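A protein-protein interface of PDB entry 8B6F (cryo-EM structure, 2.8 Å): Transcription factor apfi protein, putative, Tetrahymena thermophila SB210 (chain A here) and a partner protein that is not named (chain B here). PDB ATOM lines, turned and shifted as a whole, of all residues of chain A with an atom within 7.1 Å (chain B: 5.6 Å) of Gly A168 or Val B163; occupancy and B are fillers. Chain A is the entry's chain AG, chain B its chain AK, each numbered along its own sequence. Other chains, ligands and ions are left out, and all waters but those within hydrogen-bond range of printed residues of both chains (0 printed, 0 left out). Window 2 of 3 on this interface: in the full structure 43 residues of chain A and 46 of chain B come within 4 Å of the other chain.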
ATOM      1  N   GLY A 148       5.623  -6.337  15.693  1.00  0.00           N
ATOM      2  CA  GLY A 148       4.340  -6.974  15.882  1.00  0.00           C
ATOM      3  C   GLY A 148       3.484  -6.300  16.936  1.00  0.00           C
ATOM      4  O   GLY A 148       3.866  -5.322  17.577  1.00  0.00           O
ATOM      5  N   MET A 149       2.289  -6.857  17.113  1.00  0.00           N
ATOM      6  CA  MET A 149       1.354  -6.346  18.103  1.00  0.00           C
ATOM      7  C   MET A 149       1.938  -6.446  19.504  1.00  0.00           C
ATOM      8  O   MET A 149       2.569  -7.444  19.862  1.00  0.00           O
ATOM      9  CB  MET A 149       0.050  -7.136  18.042  1.00  0.00           C
ATOM     10  CG  MET A 149      -0.760  -6.917  16.786  1.00  0.00           C
ATOM     11  SD  MET A 149      -1.823  -8.318  16.396  1.00  0.00           S
ATOM     12  CE  MET A 149      -2.378  -8.815  18.025  1.00  0.00           C
ATOM     13  N   GLY A 150       1.714  -5.410  20.303  1.00  0.00           N
ATOM     14  CA  GLY A 150       2.136  -5.449  21.694  1.00  0.00           C
ATOM     15  C   GLY A 150       3.616  -5.709  21.861  1.00  0.00           C
ATOM     16  O   GLY A 150       4.012  -6.501  22.725  1.00  0.00           O
ATOM     17  N   SER A 151       4.442  -5.058  21.052  1.00  0.00           N
ATOM     18  CA  SER A 151       5.884  -5.247  21.068  1.00  0.00           C
ATOM     19  C   SER A 151       6.555  -3.976  21.569  1.00  0.00           C
ATOM     20  O   SER A 151       6.144  -2.866  21.216  1.00  0.00           O
ATOM     21  CB  SER A 151       6.397  -5.603  19.673  1.00  0.00           C
ATOM     22  OG  SER A 151       7.799  -5.796  19.676  1.00  0.00           O
ATOM     23  N   THR A 152       7.584  -4.141  22.394  1.00  0.00           N
ATOM     24  CA  THR A 152       8.306  -3.024  22.990  1.00  0.00           C
ATOM     25  C   THR A 152       9.736  -3.018  22.471  1.00  0.00           C
ATOM     26  O   THR A 152      10.467  -3.998  22.643  1.00  0.00           O
ATOM     27  CB  THR A 152       8.290  -3.111  24.518  1.00  0.00           C
ATOM     28  OG1 THR A 152       6.940  -3.007  24.986  1.00  0.00           O
ATOM     29  CG2 THR A 152       9.121  -1.993  25.135  1.00  0.00           C
ATOM     30  N   VAL A 165      10.271  -8.395  14.319  1.00  0.00           N
ATOM     31  CA  VAL A 165      10.068  -8.579  15.751  1.00  0.00           C
ATOM     32  C   VAL A 165       8.669  -9.146  15.939  1.00  0.00           C
ATOM     33  O   VAL A 165       7.677  -8.500  15.580  1.00  0.00           O
ATOM     34  CB  VAL A 165      10.246  -7.264  16.526  1.00  0.00           C
ATOM     35  CG1 VAL A 165       9.993  -7.477  18.011  1.00  0.00           C
ATOM     36  CG2 VAL A 165      11.638  -6.701  16.299  1.00  0.00           C
ATOM     37  N   ALA A 166       8.587 -10.349  16.496  1.00  0.00           N
ATOM     38  CA  ALA A 166       7.303 -11.012  16.652  1.00  0.00           C
ATOM     39  C   ALA A 166       6.430 -10.263  17.651  1.00  0.00           C
ATOM     40  O   ALA A 166       6.921  -9.562  18.539  1.00  0.00           O
ATOM     41  CB  ALA A 166       7.499 -12.456  17.111  1.00  0.00           C
ATOM     42  N   ALA A 167       5.118 -10.420  17.498  1.00  0.00           N
ATOM     43  CA  ALA A 167       4.180  -9.763  18.394  1.00  0.00           C
ATOM     44  C   ALA A 167       4.377 -10.257  19.820  1.00  0.00           C
ATOM     45  O   ALA A 167       4.695 -11.426  20.053  1.00  0.00           O
ATOM     46  CB  ALA A 167       2.746 -10.022  17.941  1.00  0.00           C
ATOM     47  N   GLY A 168       4.191  -9.354  20.780  1.00  0.00           N
ATOM     48  CA  GLY A 168       4.393  -9.709  22.168  1.00  0.00           C
ATOM     49  C   GLY A 168       5.838  -9.885  22.561  1.00  0.00           C
ATOM     50  O   GLY A 168       6.124 -10.580  23.538  1.00  0.00           O
ATOM     51  N   SER A 169       6.763  -9.275  21.825  1.00  0.00           N
ATOM     52  CA  SER A 169       8.191  -9.415  22.066  1.00  0.00           C
ATOM     53  C   SER A 169       8.727  -8.146  22.710  1.00  0.00           C
ATOM     54  O   SER A 169       8.447  -7.040  22.238  1.00  0.00           O
ATOM     55  CB  SER A 169       8.936  -9.691  20.760  1.00  0.00           C
ATOM     56  OG  SER A 169       8.374 -10.795  20.077  1.00  0.00           O
ATOM     57  N   VAL A 170       9.492  -8.309  23.784  1.00  0.00           N
ATOM     58  CA  VAL A 170      10.130  -7.198  24.481  1.00  0.00           C
ATOM     59  C   VAL A 170      11.607  -7.231  24.119  1.00  0.00           C
ATOM     60  O   VAL A 170      12.359  -8.080  24.612  1.00  0.00           O
ATOM     61  CB  VAL A 170       9.925  -7.283  25.999  1.00  0.00           C
ATOM     62  CG1 VAL A 170      10.585  -6.103  26.693  1.00  0.00           C
ATOM     63  CG2 VAL A 170       8.444  -7.341  26.330  1.00  0.00           C
ATOM     64  N   ALA A 184      11.872 -13.086  18.780  1.00  0.00           N
ATOM     65  CA  ALA A 184      10.629 -13.284  19.510  1.00  0.00           C
ATOM     66  C   ALA A 184      10.942 -13.627  20.959  1.00  0.00           C
ATOM     67  O   ALA A 184      12.063 -14.008  21.300  1.00  0.00           O
ATOM     68  CB  ALA A 184       9.775 -14.388  18.876  1.00  0.00           C
ATOM     69  N   GLY A 185       9.929 -13.487  21.808  1.00  0.00           N
ATOM     70  CA  GLY A 185      10.049 -13.801  23.219  1.00  0.00           C
ATOM     71  C   GLY A 185      10.209 -12.561  24.074  1.00  0.00           C
ATOM     72  O   GLY A 185      10.226 -11.422  23.598  1.00  0.00           O
ATOM     73  N   SER A 186      10.334 -12.806  25.375  1.00  0.00           N
ATOM     74  CA  SER A 186      10.486 -11.738  26.363  1.00  0.00           C
ATOM     75  C   SER A 186      11.368 -12.268  27.486  1.00  0.00           C
ATOM     76  O   SER A 186      10.897 -13.018  28.355  1.00  0.00           O
ATOM     77  CB  SER A 186       9.136 -11.276  26.903  1.00  0.00           C
ATOM     78  OG  SER A 186       9.291 -10.237  27.854  1.00  0.00           O
ATOM     79  N   CYS B 144      -2.652  -8.845  27.599  1.00  0.00           N
ATOM     80  CA  CYS B 144      -2.521 -10.067  26.823  1.00  0.00           C
ATOM     81  C   CYS B 144      -2.321  -9.750  25.345  1.00  0.00           C
ATOM     82  O   CYS B 144      -2.632  -8.659  24.866  1.00  0.00           O
ATOM     83  CB  CYS B 144      -3.756 -10.948  26.994  1.00  0.00           C
ATOM     84  SG  CYS B 144      -3.833 -11.805  28.567  1.00  0.00           S
ATOM     85  N   VAL B 145      -1.790 -10.731  24.618  1.00  0.00           N
ATOM     86  CA  VAL B 145      -1.642 -10.614  23.172  1.00  0.00           C
ATOM     87  C   VAL B 145      -2.084 -11.914  22.518  1.00  0.00           C
ATOM     88  O   VAL B 145      -1.331 -12.893  22.489  1.00  0.00           O
ATOM     89  CB  VAL B 145      -0.191 -10.275  22.790  1.00  0.00           C
ATOM     90  CG1 VAL B 145      -0.057 -10.105  21.286  1.00  0.00           C
ATOM     91  CG2 VAL B 145       0.274  -9.025  23.513  1.00  0.00           C
ATOM     92  N   ILE B 146      -3.305 -11.937  21.993  1.00  0.00           N
ATOM     93  CA  ILE B 146      -3.846 -13.101  21.304  1.00  0.00           C
ATOM     94  C   ILE B 146      -3.630 -12.884  19.813  1.00  0.00           C
ATOM     95  O   ILE B 146      -4.123 -11.901  19.248  1.00  0.00           O
ATOM     96  CB  ILE B 146      -5.334 -13.307  21.622  1.00  0.00           C
ATOM     97  CG1 ILE B 146      -5.617 -13.039  23.103  1.00  0.00           C
ATOM     98  CG2 ILE B 146      -5.737 -14.731  21.297  1.00  0.00           C
ATOM     99  CD1 ILE B 146      -4.788 -13.859  24.065  1.00  0.00           C
ATOM    100  N   LEU B 147      -2.906 -13.791  19.167  1.00  0.00           N
ATOM    101  CA  LEU B 147      -2.535 -13.619  17.772  1.00  0.00           C
ATOM    102  C   LEU B 147      -3.498 -14.362  16.851  1.00  0.00           C
ATOM    103  O   LEU B 147      -4.276 -15.216  17.279  1.00  0.00           O
ATOM    104  CB  LEU B 147      -1.096 -14.089  17.547  1.00  0.00           C
ATOM    105  CG  LEU B 147      -0.061 -13.393  18.443  1.00  0.00           C
ATOM    106  CD1 LEU B 147       1.343 -13.886  18.169  1.00  0.00           C
ATOM    107  CD2 LEU B 147      -0.112 -11.883  18.281  1.00  0.00           C
ATOM    108  N   ASN B 161       0.140 -10.909  31.360  1.00  0.00           N
ATOM    109  CA  ASN B 161       1.198 -10.564  30.410  1.00  0.00           C
ATOM    110  C   ASN B 161       1.576 -11.737  29.517  1.00  0.00           C
ATOM    111  O   ASN B 161       2.752 -11.929  29.198  1.00  0.00           O
ATOM    112  CB  ASN B 161       2.425 -10.042  31.153  1.00  0.00           C
ATOM    113  CG  ASN B 161       2.241  -8.625  31.656  1.00  0.00           C
ATOM    114  OD1 ASN B 161       1.119  -8.135  31.764  1.00  0.00           O
ATOM    115  ND2 ASN B 161       3.345  -7.957  31.961  1.00  0.00           N
ATOM    116  N   SER B 162       0.604 -12.534  29.097  1.00  0.00           N
ATOM    117  CA  SER B 162       0.855 -13.715  28.288  1.00  0.00           C
ATOM    118  C   SER B 162       0.492 -13.469  26.828  1.00  0.00           C
ATOM    119  O   SER B 162      -0.257 -12.549  26.491  1.00  0.00           O
ATOM    120  CB  SER B 162       0.088 -14.917  28.839  1.00  0.00           C
ATOM    121  OG  SER B 162      -1.167 -14.525  29.352  1.00  0.00           O
ATOM    122  N   VAL B 163       1.048 -14.309  25.959  1.00  0.00           N
ATOM    123  CA  VAL B 163       0.843 -14.236  24.519  1.00  0.00           C
ATOM    124  C   VAL B 163       0.349 -15.593  24.039  1.00  0.00           C
ATOM    125  O   VAL B 163       0.982 -16.617  24.314  1.00  0.00           O
ATOM    126  CB  VAL B 163       2.131 -13.835  23.775  1.00  0.00           C
ATOM    127  CG1 VAL B 163       1.860 -13.670  22.287  1.00  0.00           C
ATOM    128  CG2 VAL B 163       2.706 -12.557  24.360  1.00  0.00           C
ATOM    129  N   VAL B 164      -0.772 -15.596  23.325  1.00  0.00           N
ATOM    130  CA  VAL B 164      -1.300 -16.798  22.684  1.00  0.00           C
ATOM    131  C   VAL B 164      -0.818 -16.795  21.234  1.00  0.00           C
ATOM    132  O   VAL B 164      -1.284 -15.961  20.442  1.00  0.00           O
ATOM    133  CB  VAL B 164      -2.831 -16.847  22.760  1.00  0.00           C
ATOM    134  CG1 VAL B 164      -3.381 -18.021  21.957  1.00  0.00           C
ATOM    135  CG2 VAL B 164      -3.287 -16.937  24.205  1.00  0.00           C
ATOM    136  N   PRO B 165       0.088 -17.690  20.844  1.00  0.00           N
ATOM    137  CA  PRO B 165       0.634 -17.654  19.482  1.00  0.00           C
ATOM    138  C   PRO B 165      -0.445 -17.909  18.446  1.00  0.00           C
ATOM    139  O   PRO B 165      -1.538 -18.392  18.778  1.00  0.00           O
ATOM    140  CB  PRO B 165       1.679 -18.780  19.486  1.00  0.00           C
ATOM    141  CG  PRO B 165       2.030 -18.971  20.908  1.00  0.00           C
ATOM    142  CD  PRO B 165       0.780 -18.688  21.679  1.00  0.00           C
ATOM    143  N   GLY B 178       2.161 -16.996  30.788  1.00  0.00           N
ATOM    144  CA  GLY B 178       3.487 -16.860  30.222  1.00  0.00           C
ATOM    145  C   GLY B 178       3.459 -16.525  28.740  1.00  0.00           C
ATOM    146  O   GLY B 178       2.418 -16.514  28.082  1.00  0.00           O
ATOM    147  N   ASN B 179       4.652 -16.253  28.218  1.00  0.00           N
ATOM    148  CA  ASN B 179       4.843 -15.867  26.821  1.00  0.00           C
ATOM    149  C   ASN B 179       5.994 -16.685  26.251  1.00  0.00           C
ATOM    150  O   ASN B 179       7.167 -16.385  26.534  1.00  0.00           O
ATOM    151  CB  ASN B 179       5.126 -14.375  26.704  1.00  0.00           C
ATOM    152  CG  ASN B 179       5.531 -13.964  25.304  1.00  0.00           C
ATOM    153  OD1 ASN B 179       5.274 -14.675  24.335  1.00  0.00           O
ATOM    154  ND2 ASN B 179       6.164 -12.804  25.192  1.00  0.00           N
ATOM    155  N   PRO B 180       5.712 -17.721  25.449  1.00  0.00           N
ATOM    156  CA  PRO B 180       4.388 -18.203  25.018  1.00  0.00           C
ATOM    157  C   PRO B 180       3.582 -18.785  26.170  1.00  0.00           C
ATOM    158  O   PRO B 180       4.137 -19.210  27.177  1.00  0.00           O
ATOM    159  CB  PRO B 180       4.729 -19.279  23.972  1.00  0.00           C
ATOM    160  CG  PRO B 180       6.146 -19.013  23.563  1.00  0.00           C
ATOM    161  CD  PRO B 180       6.800 -18.463  24.790  1.00  0.00           C
ATOM    162  N   CYS B 181       2.261 -18.812  26.037  1.00  0.00           N
ATOM    163  CA  CYS B 181       1.404 -19.314  27.100  1.00  0.00           C
ATOM    164  C   CYS B 181       1.643 -20.803  27.322  1.00  0.00           C
ATOM    165  O   CYS B 181       1.824 -21.570  26.373  1.00  0.00           O
ATOM    166  CB  CYS B 181      -0.064 -19.059  26.762  1.00  0.00           C
ATOM    167  SG  CYS B 181      -0.618 -19.850  25.239  1.00  0.00           S
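O of Gly A168 sits at hydrogen-bond distance from ND2 of Asn B179, at 2.8 Å.
Of the 13 printed residues of chain B, 4 touch a printed residue of chain A. Printed residues of chain B that touch a printed residue of chain A: Ile B146, Leu B147, Val B163 and Asn B179. Hydrophobic or aromatic side chains of chain B that line the printed part of chain A: Leu B147 and Val B163. Hydrophobic or aromatic side chains of chain A within 4 Å of the printed part of chain B: Met A149 and Ala A167. Among the printed residues, 6 pairs touch across the chains.
Printed residues of chain B within 4 Å of Ala A167: Leu B147 (3.4 Å). Gly A168 touches just these residues of chain B: Val B163 and Asn B179. Of the printed residues of chain A, Leu B147 touches Met A149 (3.8 Å) and Ala A167 (3.4 Å). Val B163 touches just one residue of chain A: Gly A168. Of the printed residues of chain A, Asn B179 touches Gly A168 and Ser A186. The nearest residue of chain A that does not touch Val B163 is Ala A167 (4.3 Å). The nearest printed residue of chain B that does not touch Ala A167 is Val B163 (4.3 Å).
Ile B146 touches Met A149. Met A149 touches Leu B147. Ala A167 touches Leu B147 (CB to CD2, 3.4 Å). Val B163 touches Gly A168 (CG2 to CA, 3.97 Å). Asn B179 touches Ser A186 (ND2 to CB, 3.8 Å).
The backbone NH of Gly A168 lies within hydrogen-bond range of the backbone carbonyl oxygen of Met A149 (2.7 Å). N of Gly A168 sits close to O of Gly A150, 3.5 Å away. The backbone NH (N) of Leu B147 is in hydrogen-bond range of the backbone carbonyl oxygen (O) of Val B164. The backbone NH of Val B163 lies within hydrogen-bond range of the backbone carbonyl oxygen of Gly B178 (3.4 Å). The backbone carbonyl oxygen (O) of Val B163 sits at hydrogen-bond distance from the backbone NH (N) of Cys B181, 3.1 Å away.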
